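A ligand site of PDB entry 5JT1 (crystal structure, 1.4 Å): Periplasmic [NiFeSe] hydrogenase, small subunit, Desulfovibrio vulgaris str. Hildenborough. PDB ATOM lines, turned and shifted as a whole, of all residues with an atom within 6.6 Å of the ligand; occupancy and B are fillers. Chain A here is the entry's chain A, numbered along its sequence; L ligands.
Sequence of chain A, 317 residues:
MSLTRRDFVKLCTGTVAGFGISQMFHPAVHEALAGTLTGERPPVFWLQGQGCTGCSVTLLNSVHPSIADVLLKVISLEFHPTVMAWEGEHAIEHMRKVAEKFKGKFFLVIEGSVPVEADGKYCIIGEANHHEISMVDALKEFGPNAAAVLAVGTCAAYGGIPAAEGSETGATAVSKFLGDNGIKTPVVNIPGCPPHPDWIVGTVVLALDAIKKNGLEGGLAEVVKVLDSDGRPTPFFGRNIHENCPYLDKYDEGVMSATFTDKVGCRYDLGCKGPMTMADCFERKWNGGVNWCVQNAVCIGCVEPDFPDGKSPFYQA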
ATOM      1  N   ILE A 241      16.101  -2.401 -18.658  1.00  0.00           N
ATOM      2  CA  ILE A 241      16.398  -2.418 -17.224  1.00  0.00           C
ATOM      3  C   ILE A 241      17.893  -2.256 -16.981  1.00  0.00           C
ATOM      4  O   ILE A 241      18.320  -1.410 -16.178  1.00  0.00           O
ATOM      5  CB  ILE A 241      15.881  -3.721 -16.582  1.00  0.00           C
ATOM      6  CG1 ILE A 241      14.352  -3.742 -16.572  1.00  0.00           C
ATOM      7  CG2 ILE A 241      16.415  -3.834 -15.166  1.00  0.00           C
ATOM      8  CD1 ILE A 241      13.727  -4.875 -15.815  1.00  0.00           C
ATOM      9  N   HIS A 242      18.705  -3.090 -17.618  1.00  0.00           N
ATOM     10  CA  HIS A 242      20.136  -3.129 -17.327  1.00  0.00           C
ATOM     11  C   HIS A 242      20.825  -1.789 -17.597  1.00  0.00           C
ATOM     12  O   HIS A 242      21.656  -1.350 -16.789  1.00  0.00           O
ATOM     13  CB  HIS A 242      20.723  -4.241 -18.181  1.00  0.00           C
ATOM     14  CG  HIS A 242      22.216  -4.350 -18.174  1.00  0.00           C
ATOM     15  ND1 HIS A 242      22.909  -4.950 -17.140  1.00  0.00           N
ATOM     16  CD2 HIS A 242      23.142  -3.998 -19.099  1.00  0.00           C
ATOM     17  CE1 HIS A 242      24.203  -4.926 -17.427  1.00  0.00           C
ATOM     18  NE2 HIS A 242      24.371  -4.355 -18.609  1.00  0.00           N
ATOM     19  N   GLU A 243      20.518  -1.130 -18.712  1.00  0.00           N
ATOM     20  CA  GLU A 243      21.204   0.119 -19.034  1.00  0.00           C
ATOM     21  C   GLU A 243      20.836   1.225 -18.063  1.00  0.00           C
ATOM     22  O   GLU A 243      21.549   2.233 -18.018  1.00  0.00           O
ATOM     23  CB  GLU A 243      20.941   0.554 -20.475  1.00  0.00           C
ATOM     24  CG  GLU A 243      21.437  -0.440 -21.524  1.00  0.00           C
ATOM     25  CD  GLU A 243      22.943  -0.677 -21.494  1.00  0.00           C
ATOM     26  OE1 GLU A 243      23.710   0.213 -21.059  1.00  0.00           O
ATOM     27  OE2 GLU A 243      23.393  -1.776 -21.899  1.00  0.00           O
ATOM     28  N   CYS A 245      20.259   0.390 -14.669  1.00  0.00           N
ATOM     29  CA  CYS A 245      20.278  -0.300 -13.385  1.00  0.00           C
ATOM     30  C   CYS A 245      21.289   0.355 -12.438  1.00  0.00           C
ATOM     31  O   CYS A 245      22.403   0.694 -12.858  1.00  0.00           O
ATOM     32  CB  CYS A 245      20.694  -1.765 -13.576  1.00  0.00           C
ATOM     33  SG  CYS A 245      20.726  -2.720 -12.033  1.00  0.00           S
ATOM     34  N   PRO A 246      20.964   0.461 -11.146  1.00  0.00           N
ATOM     35  CA  PRO A 246      21.922   1.051 -10.206  1.00  0.00           C
ATOM     36  C   PRO A 246      23.147   0.194  -9.948  1.00  0.00           C
ATOM     37  O   PRO A 246      24.120   0.702  -9.376  1.00  0.00           O
ATOM     38  CB  PRO A 246      21.096   1.287  -8.939  1.00  0.00           C
ATOM     39  CG  PRO A 246      19.985   0.337  -9.014  1.00  0.00           C
ATOM     40  CD  PRO A 246      19.666   0.172 -10.498  1.00  0.00           C
ATOM     41  N   TYR A 247      23.163  -1.077 -10.365  1.00  0.00           N
ATOM     42  CA  TYR A 247      24.322  -1.934 -10.179  1.00  0.00           C
ATOM     43  C   TYR A 247      25.159  -2.036 -11.452  1.00  0.00           C
ATOM     44  O   TYR A 247      26.101  -2.850 -11.488  1.00  0.00           O
ATOM     45  CB  TYR A 247      23.906  -3.313  -9.653  1.00  0.00           C
ATOM     46  CG  TYR A 247      22.964  -3.180  -8.463  1.00  0.00           C
ATOM     47  CD1 TYR A 247      23.403  -2.661  -7.253  1.00  0.00           C
ATOM     48  CD2 TYR A 247      21.630  -3.519  -8.575  1.00  0.00           C
ATOM     49  CE1 TYR A 247      22.510  -2.492  -6.193  1.00  0.00           C
ATOM     50  CE2 TYR A 247      20.760  -3.371  -7.546  1.00  0.00           C
ATOM     51  CZ  TYR A 247      21.183  -2.851  -6.354  1.00  0.00           C
ATOM     52  OH  TYR A 247      20.228  -2.719  -5.365  1.00  0.00           O
ATOM     53  N   LEU A 248      24.865  -1.201 -12.465  1.00  0.00           N
ATOM     54  CA  LEU A 248      25.551  -1.293 -13.751  1.00  0.00           C
ATOM     55  C   LEU A 248      27.054  -1.050 -13.609  1.00  0.00           C
ATOM     56  O   LEU A 248      27.865  -1.683 -14.307  1.00  0.00           O
ATOM     57  CB  LEU A 248      24.921  -0.301 -14.741  1.00  0.00           C
ATOM     58  CG  LEU A 248      25.501  -0.337 -16.152  1.00  0.00           C
ATOM     59  CD1 LEU A 248      25.319  -1.701 -16.839  1.00  0.00           C
ATOM     60  CD2 LEU A 248      24.852   0.769 -16.990  1.00  0.00           C
ATOM     61  N   ASP A 249      27.460  -0.155 -12.717  1.00  0.00           N
ATOM     62  CA  ASP A 249      28.898   0.025 -12.500  1.00  0.00           C
ATOM     63  C   ASP A 249      29.566  -1.260 -12.010  1.00  0.00           C
ATOM     64  O   ASP A 249      30.679  -1.567 -12.423  1.00  0.00           O
ATOM     65  CB  ASP A 249      29.188   1.223 -11.595  1.00  0.00           C
ATOM     66  CG  ASP A 249      28.529   1.122 -10.212  1.00  0.00           C
ATOM     67  OD1 ASP A 249      27.545   0.362 -10.007  1.00  0.00           O
ATOM     68  OD2 ASP A 249      28.995   1.861  -9.300  1.00  0.00           O
ATOM     69  N   LYS A 250      28.898  -2.007 -11.125  1.00  0.00           N
ATOM     70  CA  LYS A 250      29.455  -3.290 -10.663  1.00  0.00           C
ATOM     71  C   LYS A 250      29.530  -4.321 -11.790  1.00  0.00           C
ATOM     72  O   LYS A 250      30.531  -5.053 -11.913  1.00  0.00           O
ATOM     73  CB  LYS A 250      28.652  -3.834  -9.480  1.00  0.00           C
ATOM     74  CG  LYS A 250      28.622  -2.894  -8.288  1.00  0.00           C
ATOM     75  CD  LYS A 250      30.006  -2.712  -7.690  1.00  0.00           C
ATOM     76  CE  LYS A 250      29.983  -1.742  -6.543  1.00  0.00           C
ATOM     77  NZ  LYS A 250      31.360  -1.392  -6.164  1.00  0.00           N
ATOM     78  N   TYR A 251      28.507  -4.391 -12.644  1.00  0.00           N
ATOM     79  CA  TYR A 251      28.578  -5.249 -13.829  1.00  0.00           C
ATOM     80  C   TYR A 251      29.811  -4.924 -14.665  1.00  0.00           C
ATOM     81  O   TYR A 251      30.584  -5.822 -15.038  1.00  0.00           O
ATOM     82  CB  TYR A 251      27.304  -5.057 -14.670  1.00  0.00           C
ATOM     83  CG  TYR A 251      27.294  -5.840 -15.965  1.00  0.00           C
ATOM     84  CD1 TYR A 251      26.792  -7.140 -16.014  1.00  0.00           C
ATOM     85  CD2 TYR A 251      27.775  -5.292 -17.151  1.00  0.00           C
ATOM     86  CE1 TYR A 251      26.767  -7.858 -17.202  1.00  0.00           C
ATOM     87  CE2 TYR A 251      27.746  -5.987 -18.331  1.00  0.00           C
ATOM     88  CZ  TYR A 251      27.243  -7.276 -18.340  1.00  0.00           C
ATOM     89  OH  TYR A 251      27.233  -7.981 -19.531  1.00  0.00           O
ATOM     90  N   ASP A 252      30.009  -3.636 -14.974  1.00  0.00           N
ATOM     91  CA  ASP A 252      31.128  -3.247 -15.814  1.00  0.00           C
ATOM     92  C   ASP A 252      32.467  -3.556 -15.160  1.00  0.00           C
ATOM     93  O   ASP A 252      33.447  -3.830 -15.865  1.00  0.00           O
ATOM     94  CB  ASP A 252      31.036  -1.767 -16.189  1.00  0.00           C
ATOM     95  CG  ASP A 252      29.956  -1.491 -17.214  1.00  0.00           C
ATOM     96  OD1 ASP A 252      29.542  -2.403 -17.952  1.00  0.00           O
ATOM     97  OD2 ASP A 252      29.495  -0.343 -17.259  1.00  0.00           O
ATOM     98  N   MET A 256      30.567  -9.327  -8.954  1.00  0.00           N
ATOM     99  CA  MET A 256      29.342 -10.125  -9.020  1.00  0.00           C
ATOM    100  C   MET A 256      29.050 -10.739  -7.657  1.00  0.00           C
ATOM    101  O   MET A 256      29.923 -11.371  -7.067  1.00  0.00           O
ATOM    102  CB  MET A 256      29.515 -11.294  -9.992  1.00  0.00           C
ATOM    103  CG  MET A 256      29.723 -10.884 -11.416  1.00  0.00           C
ATOM    104  SD  MET A 256      28.251 -10.085 -12.054  1.00  0.00           S
ATOM    105  CE  MET A 256      28.882  -9.540 -13.653  1.00  0.00           C
ATOM    106  N   GLY A 265      27.121  -6.293  -5.026  1.00  0.00           N
ATOM    107  CA  GLY A 265      27.523  -6.707  -6.357  1.00  0.00           C
ATOM    108  C   GLY A 265      26.365  -6.769  -7.348  1.00  0.00           C
ATOM    109  O   GLY A 265      25.196  -6.708  -7.004  1.00  0.00           O
ATOM    110  N   CYS A 266      26.742  -6.872  -8.626  1.00  0.00           N
ATOM    111  CA  CYS A 266      25.759  -7.128  -9.679  1.00  0.00           C
ATOM    112  C   CYS A 266      25.236  -8.556  -9.560  1.00  0.00           C
ATOM    113  O   CYS A 266      25.940  -9.459  -9.074  1.00  0.00           O
ATOM    114  CB  CYS A 266      26.431  -6.890 -11.047  1.00  0.00           C
ATOM    115  SG  CYS A 266      25.600  -7.552 -12.531  1.00  0.00           S
ATOM    116  N   ARG A 267      23.979  -8.750  -9.949  1.00  0.00           N
ATOM    117  CA  ARG A 267      23.255 -10.019  -9.833  1.00  0.00           C
ATOM    118  C   ARG A 267      23.328 -10.901 -11.097  1.00  0.00           C
ATOM    119  O   ARG A 267      22.653 -11.931 -11.164  1.00  0.00           O
ATOM    120  CB  ARG A 267      21.781  -9.689  -9.532  1.00  0.00           C
ATOM    121  CG  ARG A 267      21.479  -9.172  -8.133  1.00  0.00           C
ATOM    122  CD  ARG A 267      21.986  -7.764  -7.833  1.00  0.00           C
ATOM    123  NE  ARG A 267      21.204  -7.154  -6.751  1.00  0.00           N
ATOM    124  CZ  ARG A 267      21.645  -6.269  -5.852  1.00  0.00           C
ATOM    125  NH1 ARG A 267      22.914  -5.856  -5.842  1.00  0.00           N
ATOM    126  NH2 ARG A 267      20.791  -5.807  -4.939  1.00  0.00           N
ATOM    127  N   TYR A 268      24.166 -10.530 -12.074  1.00  0.00           N
ATOM    128  CA  TYR A 268      24.243 -11.283 -13.331  1.00  0.00           C
ATOM    129  C   TYR A 268      24.582 -12.763 -13.126  1.00  0.00           C
ATOM    130  O   TYR A 268      23.950 -13.640 -13.730  1.00  0.00           O
ATOM    131  CB  TYR A 268      25.289 -10.635 -14.240  1.00  0.00           C
ATOM    132  CG  TYR A 268      25.402 -11.261 -15.595  1.00  0.00           C
ATOM    133  CD1 TYR A 268      24.484 -10.985 -16.579  1.00  0.00           C
ATOM    134  CD2 TYR A 268      26.438 -12.144 -15.879  1.00  0.00           C
ATOM    135  CE1 TYR A 268      24.574 -11.538 -17.828  1.00  0.00           C
ATOM    136  CE2 TYR A 268      26.553 -12.716 -17.139  1.00  0.00           C
ATOM    137  CZ  TYR A 268      25.605 -12.413 -18.101  1.00  0.00           C
ATOM    138  OH  TYR A 268      25.716 -12.974 -19.342  1.00  0.00           O
ATOM    139  N   ASP A 269      25.602 -13.076 -12.293  1.00  0.00           N
ATOM    140  CA  ASP A 269      25.956 -14.482 -12.118  1.00  0.00           C
ATOM    141  C   ASP A 269      24.865 -15.268 -11.392  1.00  0.00           C
ATOM    142  O   ASP A 269      24.807 -16.491 -11.542  1.00  0.00           O
ATOM    143  CB  ASP A 269      27.263 -14.649 -11.333  1.00  0.00           C
ATOM    144  CG  ASP A 269      28.501 -14.269 -12.126  1.00  0.00           C
ATOM    145  OD1 ASP A 269      28.391 -14.028 -13.352  1.00  0.00           O
ATOM    146  OD2 ASP A 269      29.599 -14.258 -11.507  1.00  0.00           O
ATOM    147  N   CYS A 272      20.362 -12.783 -13.205  1.00  0.00           N
ATOM    148  CA  CYS A 272      19.596 -11.610 -13.600  1.00  0.00           C
ATOM    149  C   CYS A 272      19.485 -11.475 -15.120  1.00  0.00           C
ATOM    150  O   CYS A 272      20.487 -11.466 -15.836  1.00  0.00           O
ATOM    151  CB  CYS A 272      20.259 -10.368 -13.028  1.00  0.00           C
ATOM    152  SG  CYS A 272      19.296  -8.815 -13.318  1.00  0.00           S
ATOM    153  N   LYS A 273      18.252 -11.309 -15.599  1.00  0.00           N
ATOM    154  CA  LYS A 273      17.940 -11.139 -17.028  1.00  0.00           C
ATOM    155  C   LYS A 273      17.673  -9.681 -17.410  1.00  0.00           C
ATOM    156  O   LYS A 273      17.163  -9.419 -18.511  1.00  0.00           O
ATOM    157  CB  LYS A 273      16.764 -12.043 -17.454  1.00  0.00           C
ATOM    158  CG  LYS A 273      16.967 -13.539 -17.160  1.00  0.00           C
ATOM    159  CD  LYS A 273      18.298 -14.070 -17.677  1.00  0.00           C
ATOM    160  CE  LYS A 273      18.454 -15.592 -17.527  1.00  0.00           C
ATOM    161  NZ  LYS A 273      18.095 -16.081 -16.210  1.00  0.00           N
ATOM    162  N   GLY A 274      18.040  -8.728 -16.550  1.00  0.00           N
ATOM    163  CA  GLY A 274      17.935  -7.320 -16.886  1.00  0.00           C
ATOM    164  C   GLY A 274      18.483  -6.939 -18.256  1.00  0.00           C
ATOM    165  O   GLY A 274      17.873  -6.091 -18.930  1.00  0.00           O
ATOM    166  N   PRO A 275      19.610  -7.501 -18.694  1.00  0.00           N
ATOM    167  CA  PRO A 275      20.144  -7.103 -20.003  1.00  0.00           C
ATOM    168  C   PRO A 275      19.198  -7.319 -21.165  1.00  0.00           C
ATOM    169  O   PRO A 275      19.284  -6.595 -22.171  1.00  0.00           O
ATOM    170  CB  PRO A 275      21.423  -7.949 -20.137  1.00  0.00           C
ATOM    171  CG  PRO A 275      21.859  -8.188 -18.736  1.00  0.00           C
ATOM    172  CD  PRO A 275      20.580  -8.333 -17.943  1.00  0.00           C
ATOM    173  N   TRP A 292      12.044  -3.899  -5.504  1.00  0.00           N
ATOM    174  CA  TRP A 292      11.883  -4.433  -6.857  1.00  0.00           C
ATOM    175  C   TRP A 292      12.786  -5.645  -7.020  1.00  0.00           C
ATOM    176  O   TRP A 292      13.616  -5.954  -6.165  1.00  0.00           O
ATOM    177  CB  TRP A 292      12.153  -3.390  -7.949  1.00  0.00           C
ATOM    178  CG  TRP A 292      13.578  -2.882  -8.068  1.00  0.00           C
ATOM    179  CD1 TRP A 292      14.335  -2.258  -7.108  1.00  0.00           C
ATOM    180  CD2 TRP A 292      14.375  -2.912  -9.262  1.00  0.00           C
ATOM    181  NE1 TRP A 292      15.552  -1.917  -7.641  1.00  0.00           N
ATOM    182  CE2 TRP A 292      15.613  -2.316  -8.953  1.00  0.00           C
ATOM    183  CE3 TRP A 292      14.155  -3.390 -10.563  1.00  0.00           C
ATOM    184  CZ2 TRP A 292      16.626  -2.150  -9.909  1.00  0.00           C
ATOM    185  CZ3 TRP A 292      15.160  -3.230 -11.518  1.00  0.00           C
ATOM    186  CH2 TRP A 292      16.383  -2.607 -11.180  1.00  0.00           C
ATOM    187  N   VAL A 294      15.294  -6.749  -8.871  1.00  0.00           N
ATOM    188  CA  VAL A 294      16.752  -6.746  -8.921  1.00  0.00           C
ATOM    189  C   VAL A 294      17.377  -6.448  -7.568  1.00  0.00           C
ATOM    190  O   VAL A 294      18.384  -7.042  -7.190  1.00  0.00           O
ATOM    191  CB  VAL A 294      17.256  -5.775 -10.013  1.00  0.00           C
ATOM    192  CG1 VAL A 294      18.794  -5.594  -9.939  1.00  0.00           C
ATOM    193  CG2 VAL A 294      16.844  -6.275 -11.400  1.00  0.00           C
ATOM    194  N   ALA A 297      16.389  -9.868  -5.417  1.00  0.00           N
ATOM    195  CA  ALA A 297      16.908 -11.142  -5.893  1.00  0.00           C
ATOM    196  C   ALA A 297      17.448 -10.943  -7.303  1.00  0.00           C
ATOM    197  O   ALA A 297      18.542 -10.376  -7.450  1.00  0.00           O
ATOM    198  CB  ALA A 297      15.820 -12.224  -5.855  1.00  0.00           C
ATOM    199  N   CYS A 299      16.072 -10.154 -11.697  1.00  0.00           N
ATOM    200  CA  CYS A 299      15.035 -10.034 -12.721  1.00  0.00           C
ATOM    201  C   CYS A 299      14.944 -11.342 -13.506  1.00  0.00           C
ATOM    202  O   CYS A 299      15.966 -11.933 -13.879  1.00  0.00           O
ATOM    203  CB  CYS A 299      15.350  -8.878 -13.667  1.00  0.00           C
ATOM    204  SG  CYS A 299      14.209  -8.629 -15.098  1.00  0.00           S
HETATM  205 FE1  LIG L   1      20.967  -7.232 -13.497  1.00  0.00          FE
HETATM  206 FE2  LIG L   1      22.351  -5.638 -15.273  1.00  0.00          FE
HETATM  207 FE3  LIG L   1      23.609  -6.495 -13.034  1.00  0.00          FE
HETATM  208 FE4  LIG L   1      21.604  -4.656 -12.887  1.00  0.00          FE
HETATM  209  S1  LIG L   1      23.659  -4.379 -13.836  1.00  0.00           S
HETATM  210  S2  LIG L   1      21.923  -6.453 -11.504  1.00  0.00           S
HETATM  211  S3  LIG L   1      20.184  -5.372 -14.590  1.00  0.00           S
HETATM  212  S4  LIG L   1      22.800  -7.839 -14.743  1.00  0.00           S
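A ring nitrogen (ND1) of His 242 binds an iron atom (FE2) of the ligand, at 2.1 Å.
SG of Cys 245 binds FE4 of the ligand (2.3 Å).
An iron atom (FE1) of the ligand is bound by the side-chain sulfur (SG) of Cys 272 (2.3 Å).
An iron atom (FE3) of the ligand is bound by the side-chain sulfur (SG) of Cys 266, at 2.3 Å.
A sulfur (S2) of the ligand lies close to the backbone NH of Arg 267, 3.5 Å away.
N of Leu 248 sits close to S1 of the ligand (3.7 Å).
The backbone NH (N) of His 242 lies within hydrogen-bond range of the backbone carbonyl oxygen (O) of Gly 274 (3.4 Å).
SG of Cys 245 lies close to N of Tyr 247.
N of Cys 272 lies within hydrogen-bond range of O of Arg 267, at 3.2 Å.
SG of Cys 272 lies close to N of Gly 274.
SD of Met 256 sits close to SG of Cys 266 (3.7 Å).
The backbone carbonyl oxygen (O) of Val 294 is in hydrogen-bond range of the guanidinium group (NE) of Arg 267 (2.9 Å).
The guanidinium group (NH2) of Arg 267 sits at hydrogen-bond distance from the side-chain hydroxyl (OH) of Tyr 247, at 3.2 Å.
The guanidinium group (NH1) of Arg 267 is in hydrogen-bond range of the backbone carbonyl oxygen (O) of Gly 265, at 2.7 Å.
O of Tyr 247 lies close to S1 of the ligand (3.7 Å).
Tyr 251 touches the ligand (CB to S1, 3.8 Å).
Tyr 268 touches the ligand.
Gly 274 touches the ligand.
Pro 275 touches the ligand.
Val 294 touches the ligand.
12 residues have an atom within 4 Å of the ligand: His 242, Cys 245, Tyr 247, Leu 248, Tyr 251, Cys 266, Arg 267, Tyr 268, Cys 272, Gly 274, Pro 275 and Val 294.
The nearest printed residue that does not touch the ligand is Ile 241 (4.1 Å).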
